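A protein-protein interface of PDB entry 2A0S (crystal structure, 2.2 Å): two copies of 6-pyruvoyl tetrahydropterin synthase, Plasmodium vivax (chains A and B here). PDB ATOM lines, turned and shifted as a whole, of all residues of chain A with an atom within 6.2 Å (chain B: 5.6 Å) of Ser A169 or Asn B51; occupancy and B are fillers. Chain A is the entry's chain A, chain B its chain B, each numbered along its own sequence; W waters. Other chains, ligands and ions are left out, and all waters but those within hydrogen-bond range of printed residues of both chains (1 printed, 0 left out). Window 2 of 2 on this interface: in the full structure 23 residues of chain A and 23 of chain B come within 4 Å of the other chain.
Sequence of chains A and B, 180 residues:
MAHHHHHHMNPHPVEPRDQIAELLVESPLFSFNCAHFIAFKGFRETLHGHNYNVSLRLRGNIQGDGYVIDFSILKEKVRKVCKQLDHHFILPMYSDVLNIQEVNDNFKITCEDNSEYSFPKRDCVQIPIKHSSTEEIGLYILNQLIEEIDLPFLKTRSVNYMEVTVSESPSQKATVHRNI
N of Gly A49 sits close to O of Cys B34, at 3.4 Å.
ND1 of His A50 is in hydrogen-bond range of OD1 of Asn B51, 2.8 Å away.
The side-chain amide oxygen of Asn A51 is in hydrogen-bond range of a ring nitrogen (ND1) of His B50 (2.8 Å).
The side-chain amide nitrogen (ND2) of Asn A51 sits close to the backbone NH (N) of Asn B51, at 3.1 Å.
The backbone carbonyl oxygen of Glu B168 lies within hydrogen-bond range of the side-chain amide nitrogen of Asn A51, 2.9 Å away.
The backbone carbonyl oxygen (O) of Glu A168 sits at hydrogen-bond distance from the side-chain amide nitrogen (ND2) of Asn B51, at 2.9 Å.
The backbone carbonyl oxygen (O) of Gly A49 sits close to the backbone carbonyl oxygen (O) of His B50, at 3.4 Å.
O of Gly B49 sits close to O of His A50, at 3.4 Å.
O of Glu A168 is in hydrogen-bond range of ND1 of His A50 (3.3 Å).
The side-chain carboxylate of Glu A168 lies close to the side-chain amide oxygen of Gln A172 (2.9 Å).
The side-chain hydroxyl of Ser A169 is in hydrogen-bond range of the side-chain hydroxyl of Ser A171 (2.8 Å).
The side-chain amide oxygen (OD1) of Asn B51 sits close to the side-chain amide oxygen (OD1) of Asn B33 (3.0 Å).
The backbone carbonyl oxygen (O) of Cys B34 sits at hydrogen-bond distance from the backbone NH (N) of His B50, 2.9 Å away.
A ring nitrogen (ND1) of His B50 lies within hydrogen-bond range of the backbone carbonyl oxygen of Glu B168 (3.3 Å).
Among the printed residues, pairs that only touch across the chains: Gly A49 with Asn B33, Gly A49 with Gly B49, Gly A49 with Asn B51, His A50 with Asn B33, His A50 with His B50, Asn A51 with Gly B49, Asn A51 with Ser B169 and Ser A169 with Asn B51.
Printed residues of chain B within 4 Å of Asn A51: Gly B49, His B50, Asn B51, Glu B168 and Ser B169.
Ser A169 touches just one residue of chain B: Asn B51 (3.7 Å).
Printed residues of chain A within 4 Å of Gly B49: Gly A49, His A50 and Asn A51.
Asn B51 touches just these residues of chain A: Gly A49 (3.8 Å), His A50 (2.8 Å), Asn A51 (3.1 Å), Glu A168 (2.9 Å) and Ser A169 (3.7 Å).
Tyr B52 touches none of the printed residues of chain A.
Of the printed residues of chain A, Glu B168 touches Asn A51 (2.9 Å).
The nearest residue of chain B that does not touch Ser A169 is Asn B33 (5.1 Å).
Of the 11 printed residues of chain B, 7 touch a printed residue of chain A.
Printed residues of chain B that touch a printed residue of chain A: Asn B33, Cys B34, Gly B49, His B50, Asn B51, Glu B168 and Ser B169.
Hydrophobic or aromatic side chains of chain B within 4 Å of the printed part of chain A: His B50.
Hydrophobic or aromatic side chains of chain A that line the printed part of chain B: His A50.
Among the printed residues, 16 pairs touch across the chains.
Among the printed residues, no Asp or Glu carboxylate lies within 4 Å of a Lys or Arg side-chain nitrogen of the other chain.
Gly B49 touches its own counterpart, Gly A49.
Gly A49 touches His B50, and with the chains exchanged His A50 touches Gly B49.
Asn A51 touches its own counterpart, Asn B51.
Asn A51 touches Ser B169, and with the chains exchanged Ser A169 touches Asn B51.
7 positions are printed for both chains.
Water W1 lies within hydrogen-bond range of the side-chain amide nitrogen of Asn A51 and the side-chain amide nitrogen of Asn B51.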
ATOM      1  N   GLY A  49     -10.649 -25.223 -18.761  1.00  0.00           N
ATOM      2  CA  GLY A  49     -10.884 -26.647 -18.563  1.00  0.00           C
ATOM      3  C   GLY A  49     -11.477 -26.984 -17.215  1.00  0.00           C
ATOM      4  O   GLY A  49     -11.590 -26.118 -16.344  1.00  0.00           O
ATOM      5  N   HIS A  50     -11.857 -28.251 -17.052  1.00  0.00           N
ATOM      6  CA  HIS A  50     -12.467 -28.745 -15.820  1.00  0.00           C
ATOM      7  C   HIS A  50     -12.114 -30.202 -15.550  1.00  0.00           C
ATOM      8  O   HIS A  50     -11.819 -30.963 -16.474  1.00  0.00           O
ATOM      9  CB  HIS A  50     -13.993 -28.634 -15.894  1.00  0.00           C
ATOM     10  CG  HIS A  50     -14.496 -27.231 -16.015  1.00  0.00           C
ATOM     11  ND1 HIS A  50     -14.622 -26.389 -14.932  1.00  0.00           N
ATOM     12  CD2 HIS A  50     -14.910 -26.525 -17.091  1.00  0.00           C
ATOM     13  CE1 HIS A  50     -15.089 -25.221 -15.336  1.00  0.00           C
ATOM     14  NE2 HIS A  50     -15.275 -25.279 -16.642  1.00  0.00           N
ATOM     15  N   ASN A  51     -12.144 -30.575 -14.272  1.00  0.00           N
ATOM     16  CA  ASN A  51     -12.209 -31.975 -13.877  1.00  0.00           C
ATOM     17  C   ASN A  51     -13.682 -32.353 -13.777  1.00  0.00           C
ATOM     18  O   ASN A  51     -14.320 -32.139 -12.741  1.00  0.00           O
ATOM     19  CB  ASN A  51     -11.518 -32.210 -12.528  1.00  0.00           C
ATOM     20  CG  ASN A  51     -10.045 -31.843 -12.542  1.00  0.00           C
ATOM     21  OD1 ASN A  51      -9.314 -32.164 -13.480  1.00  0.00           O
ATOM     22  ND2 ASN A  51      -9.597 -31.176 -11.484  1.00  0.00           N
ATOM     23  N   TYR A  52     -14.230 -32.882 -14.868  1.00  0.00           N
ATOM     24  CA  TYR A  52     -15.626 -33.312 -14.888  1.00  0.00           C
ATOM     25  C   TYR A  52     -15.786 -34.614 -14.119  1.00  0.00           C
ATOM     26  O   TYR A  52     -14.888 -35.455 -14.120  1.00  0.00           O
ATOM     27  CB  TYR A  52     -16.117 -33.511 -16.318  1.00  0.00           C
ATOM     28  CG  TYR A  52     -16.279 -32.246 -17.134  1.00  0.00           C
ATOM     29  CD1 TYR A  52     -15.223 -31.745 -17.896  1.00  0.00           C
ATOM     30  CD2 TYR A  52     -17.498 -31.570 -17.172  1.00  0.00           C
ATOM     31  CE1 TYR A  52     -15.373 -30.590 -18.663  1.00  0.00           C
ATOM     32  CE2 TYR A  52     -17.658 -30.415 -17.931  1.00  0.00           C
ATOM     33  CZ  TYR A  52     -16.592 -29.931 -18.674  1.00  0.00           C
ATOM     34  OH  TYR A  52     -16.747 -28.788 -19.427  1.00  0.00           O
ATOM     35  N   SER A 167     -20.819 -33.102 -13.035  1.00  0.00           N
ATOM     36  CA  SER A 167     -20.341 -31.890 -12.384  1.00  0.00           C
ATOM     37  C   SER A 167     -19.205 -31.258 -13.178  1.00  0.00           C
ATOM     38  O   SER A 167     -18.242 -31.934 -13.546  1.00  0.00           O
ATOM     39  CB  SER A 167     -19.896 -32.175 -10.947  1.00  0.00           C
ATOM     40  OG  SER A 167     -18.782 -33.047 -10.913  1.00  0.00           O
ATOM     41  N   GLU A 168     -19.345 -29.965 -13.455  1.00  0.00           N
ATOM     42  CA  GLU A 168     -18.295 -29.168 -14.080  1.00  0.00           C
ATOM     43  C   GLU A 168     -17.247 -28.854 -13.017  1.00  0.00           C
ATOM     44  O   GLU A 168     -16.047 -28.831 -13.291  1.00  0.00           O
ATOM     45  CB  GLU A 168     -18.889 -27.873 -14.636  1.00  0.00           C
ATOM     46  CG  GLU A 168     -18.096 -27.242 -15.772  1.00  0.00           C
ATOM     47  CD  GLU A 168     -18.750 -25.984 -16.327  1.00  0.00           C
ATOM     48  OE1 GLU A 168     -19.424 -25.266 -15.556  1.00  0.00           O
ATOM     49  OE2 GLU A 168     -18.584 -25.707 -17.536  1.00  0.00           O
ATOM     50  N   SER A 169     -17.728 -28.614 -11.801  1.00  0.00           N
ATOM     51  CA  SER A 169     -16.892 -28.387 -10.632  1.00  0.00           C
ATOM     52  C   SER A 169     -17.632 -28.959  -9.418  1.00  0.00           C
ATOM     53  O   SER A 169     -18.828 -29.248  -9.515  1.00  0.00           O
ATOM     54  CB  SER A 169     -16.629 -26.888 -10.450  1.00  0.00           C
ATOM     55  OG  SER A 169     -17.833 -26.178 -10.206  1.00  0.00           O
ATOM     56  N   PRO A 170     -16.931 -29.142  -8.278  1.00  0.00           N
ATOM     57  CA  PRO A 170     -17.612 -29.592  -7.055  1.00  0.00           C
ATOM     58  C   PRO A 170     -18.798 -28.706  -6.648  1.00  0.00           C
ATOM     59  O   PRO A 170     -19.599 -29.101  -5.797  1.00  0.00           O
ATOM     60  CB  PRO A 170     -16.509 -29.514  -5.994  1.00  0.00           C
ATOM     61  CG  PRO A 170     -15.247 -29.675  -6.758  1.00  0.00           C
ATOM     62  CD  PRO A 170     -15.481 -28.975  -8.062  1.00  0.00           C
ATOM     63  N   SER A 171     -18.905 -27.532  -7.267  1.00  0.00           N
ATOM     64  CA  SER A 171     -19.956 -26.565  -6.951  1.00  0.00           C
ATOM     65  C   SER A 171     -21.120 -26.556  -7.946  1.00  0.00           C
ATOM     66  O   SER A 171     -22.250 -26.238  -7.575  1.00  0.00           O
ATOM     67  CB  SER A 171     -19.364 -25.158  -6.831  1.00  0.00           C
ATOM     68  OG  SER A 171     -18.796 -24.737  -8.060  1.00  0.00           O
ATOM     69  N   GLN A 172     -20.839 -26.904  -9.201  1.00  0.00           N
ATOM     70  CA  GLN A 172     -21.829 -26.818 -10.280  1.00  0.00           C
ATOM     71  C   GLN A 172     -22.162 -28.187 -10.874  1.00  0.00           C
ATOM     72  O   GLN A 172     -21.303 -28.836 -11.475  1.00  0.00           O
ATOM     73  CB  GLN A 172     -21.334 -25.878 -11.382  1.00  0.00           C
ATOM     74  CG  GLN A 172     -21.145 -24.432 -10.942  1.00  0.00           C
ATOM     75  CD  GLN A 172     -20.423 -23.584 -11.978  1.00  0.00           C
ATOM     76  OE1 GLN A 172     -20.360 -23.935 -13.157  1.00  0.00           O
ATOM     77  NE2 GLN A 172     -19.876 -22.458 -11.538  1.00  0.00           N
ATOM     78  N   LYS A 173     -23.415 -28.609 -10.711  1.00  0.00           N
ATOM     79  CA  LYS A 173     -23.866 -29.923 -11.173  1.00  0.00           C
ATOM     80  C   LYS A 173     -25.114 -29.843 -12.053  1.00  0.00           C
ATOM     81  O   LYS A 173     -25.985 -28.997 -11.837  1.00  0.00           O
ATOM     82  CB  LYS A 173     -24.148 -30.846  -9.983  1.00  0.00           C
ATOM     83  CG  LYS A 173     -22.927 -31.217  -9.157  1.00  0.00           C
ATOM     84  CD  LYS A 173     -23.285 -32.203  -8.052  1.00  0.00           C
ATOM     85  CE  LYS A 173     -22.053 -32.648  -7.274  1.00  0.00           C
ATOM     86  NZ  LYS A 173     -21.402 -31.527  -6.538  1.00  0.00           N
ATOM     87  N   PHE B  32      -8.672 -22.122  -9.903  1.00  0.00           N
ATOM     88  CA  PHE B  32      -8.555 -21.641 -11.272  1.00  0.00           C
ATOM     89  C   PHE B  32      -8.796 -22.777 -12.260  1.00  0.00           C
ATOM     90  O   PHE B  32      -8.058 -23.764 -12.294  1.00  0.00           O
ATOM     91  CB  PHE B  32      -7.235 -20.888 -11.528  1.00  0.00           C
ATOM     92  CG  PHE B  32      -5.990 -21.628 -11.111  1.00  0.00           C
ATOM     93  CD1 PHE B  32      -5.199 -22.268 -12.060  1.00  0.00           C
ATOM     94  CD2 PHE B  32      -5.580 -21.643  -9.781  1.00  0.00           C
ATOM     95  CE1 PHE B  32      -4.032 -22.932 -11.691  1.00  0.00           C
ATOM     96  CE2 PHE B  32      -4.419 -22.310  -9.400  1.00  0.00           C
ATOM     97  CZ  PHE B  32      -3.641 -22.955 -10.357  1.00  0.00           C
ATOM     98  N   ASN B  33      -9.868 -22.635 -13.033  1.00  0.00           N
ATOM     99  CA  ASN B  33     -10.256 -23.628 -14.022  1.00  0.00           C
ATOM    100  C   ASN B  33      -9.559 -23.321 -15.338  1.00  0.00           C
ATOM    101  O   ASN B  33      -9.883 -22.338 -16.010  1.00  0.00           O
ATOM    102  CB  ASN B  33     -11.779 -23.651 -14.186  1.00  0.00           C
ATOM    103  CG  ASN B  33     -12.511 -23.866 -12.866  1.00  0.00           C
ATOM    104  OD1 ASN B  33     -11.954 -24.407 -11.908  1.00  0.00           O
ATOM    105  ND2 ASN B  33     -13.764 -23.435 -12.811  1.00  0.00           N
ATOM    106  N   CYS B  34      -8.588 -24.160 -15.692  1.00  0.00           N
ATOM    107  CA  CYS B  34      -7.673 -23.856 -16.789  1.00  0.00           C
ATOM    108  C   CYS B  34      -7.444 -25.006 -17.758  1.00  0.00           C
ATOM    109  O   CYS B  34      -7.643 -26.172 -17.417  1.00  0.00           O
ATOM    110  CB  CYS B  34      -6.324 -23.405 -16.226  1.00  0.00           C
ATOM    111  SG  CYS B  34      -6.368 -21.795 -15.437  1.00  0.00           S
ATOM    112  N   GLY B  49      -7.822 -30.051 -19.488  1.00  0.00           N
ATOM    113  CA  GLY B  49      -7.979 -29.034 -18.454  1.00  0.00           C
ATOM    114  C   GLY B  49      -8.224 -29.602 -17.075  1.00  0.00           C
ATOM    115  O   GLY B  49      -8.423 -30.810 -16.919  1.00  0.00           O
ATOM    116  N   HIS B  50      -8.207 -28.719 -16.077  1.00  0.00           N
ATOM    117  CA  HIS B  50      -8.406 -29.094 -14.680  1.00  0.00           C
ATOM    118  C   HIS B  50      -9.097 -27.994 -13.887  1.00  0.00           C
ATOM    119  O   HIS B  50      -9.004 -26.813 -14.230  1.00  0.00           O
ATOM    120  CB  HIS B  50      -7.063 -29.390 -14.007  1.00  0.00           C
ATOM    121  CG  HIS B  50      -6.336 -30.560 -14.586  1.00  0.00           C
ATOM    122  ND1 HIS B  50      -6.659 -31.863 -14.278  1.00  0.00           N
ATOM    123  CD2 HIS B  50      -5.301 -30.623 -15.455  1.00  0.00           C
ATOM    124  CE1 HIS B  50      -5.854 -32.681 -14.934  1.00  0.00           C
ATOM    125  NE2 HIS B  50      -5.018 -31.953 -15.653  1.00  0.00           N
ATOM    126  N   ASN B  51      -9.791 -28.396 -12.826  1.00  0.00           N
ATOM    127  CA  ASN B  51     -10.184 -27.478 -11.767  1.00  0.00           C
ATOM    128  C   ASN B  51      -9.062 -27.475 -10.736  1.00  0.00           C
ATOM    129  O   ASN B  51      -9.018 -28.336  -9.852  1.00  0.00           O
ATOM    130  CB  ASN B  51     -11.501 -27.909 -11.109  1.00  0.00           C
ATOM    131  CG  ASN B  51     -12.674 -27.932 -12.078  1.00  0.00           C
ATOM    132  OD1 ASN B  51     -12.834 -27.040 -12.912  1.00  0.00           O
ATOM    133  ND2 ASN B  51     -13.516 -28.952 -11.954  1.00  0.00           N
ATOM    134  N   TYR B  52      -8.135 -26.531 -10.871  1.00  0.00           N
ATOM    135  CA  TYR B  52      -7.021 -26.416  -9.932  1.00  0.00           C
ATOM    136  C   TYR B  52      -7.501 -25.794  -8.629  1.00  0.00           C
ATOM    137  O   TYR B  52      -8.401 -24.955  -8.632  1.00  0.00           O
ATOM    138  CB  TYR B  52      -5.895 -25.563 -10.512  1.00  0.00           C
ATOM    139  CG  TYR B  52      -5.105 -26.193 -11.642  1.00  0.00           C
ATOM    140  CD1 TYR B  52      -5.476 -25.996 -12.973  1.00  0.00           C
ATOM    141  CD2 TYR B  52      -3.963 -26.951 -11.382  1.00  0.00           C
ATOM    142  CE1 TYR B  52      -4.743 -26.556 -14.017  1.00  0.00           C
ATOM    143  CE2 TYR B  52      -3.223 -27.519 -12.419  1.00  0.00           C
ATOM    144  CZ  TYR B  52      -3.620 -27.317 -13.733  1.00  0.00           C
ATOM    145  OH  TYR B  52      -2.893 -27.874 -14.762  1.00  0.00           O
ATOM    146  N   ASN B  53      -6.900 -26.211  -7.519  1.00  0.00           N
ATOM    147  CA  ASN B  53      -7.260 -25.684  -6.204  1.00  0.00           C
ATOM    148  C   ASN B  53      -6.021 -25.381  -5.368  1.00  0.00           C
ATOM    149  O   ASN B  53      -5.064 -26.159  -5.356  1.00  0.00           O
ATOM    150  CB  ASN B  53      -8.182 -26.661  -5.471  1.00  0.00           C
ATOM    151  CG  ASN B  53      -9.283 -25.960  -4.699  1.00  0.00           C
ATOM    152  OD1 ASN B  53     -10.467 -26.173  -4.961  1.00  0.00           O
ATOM    153  ND2 ASN B  53      -8.902 -25.115  -3.750  1.00  0.00           N
ATOM    154  N   SER B 167      -3.571 -28.475  -6.155  1.00  0.00           N
ATOM    155  CA  SER B 167      -4.098 -29.746  -6.637  1.00  0.00           C
ATOM    156  C   SER B 167      -4.538 -29.635  -8.092  1.00  0.00           C
ATOM    157  O   SER B 167      -5.271 -28.717  -8.459  1.00  0.00           O
ATOM    158  CB  SER B 167      -5.257 -30.232  -5.761  1.00  0.00           C
ATOM    159  OG  SER B 167      -6.359 -29.347  -5.823  1.00  0.00           O
ATOM    160  N   GLU B 168      -4.060 -30.567  -8.912  1.00  0.00           N
ATOM    161  CA  GLU B 168      -4.482 -30.694 -10.302  1.00  0.00           C
ATOM    162  C   GLU B 168      -5.857 -31.355 -10.315  1.00  0.00           C
ATOM    163  O   GLU B 168      -6.720 -31.020 -11.127  1.00  0.00           O
ATOM    164  CB  GLU B 168      -3.475 -31.550 -11.069  1.00  0.00           C
ATOM    165  CG  GLU B 168      -3.426 -31.296 -12.566  1.00  0.00           C
ATOM    166  CD  GLU B 168      -2.496 -32.254 -13.291  1.00  0.00           C
ATOM    167  OE1 GLU B 168      -2.380 -33.418 -12.852  1.00  0.00           O
ATOM    168  OE2 GLU B 168      -1.883 -31.848 -14.304  1.00  0.00           O
ATOM    169  N   SER B 169      -6.035 -32.304  -9.400  1.00  0.00           N
ATOM    170  CA  SER B 169      -7.296 -32.999  -9.188  1.00  0.00           C
ATOM    171  C   SER B 169      -7.404 -33.313  -7.692  1.00  0.00           C
ATOM    172  O   SER B 169      -6.400 -33.223  -6.978  1.00  0.00           O
ATOM    173  CB  SER B 169      -7.339 -34.286 -10.019  1.00  0.00           C
ATOM    174  OG  SER B 169      -6.313 -35.184  -9.630  1.00  0.00           O
HETATM  175  O   HOH W   1     -12.274 -30.899  -9.332  1.00  0.00           O
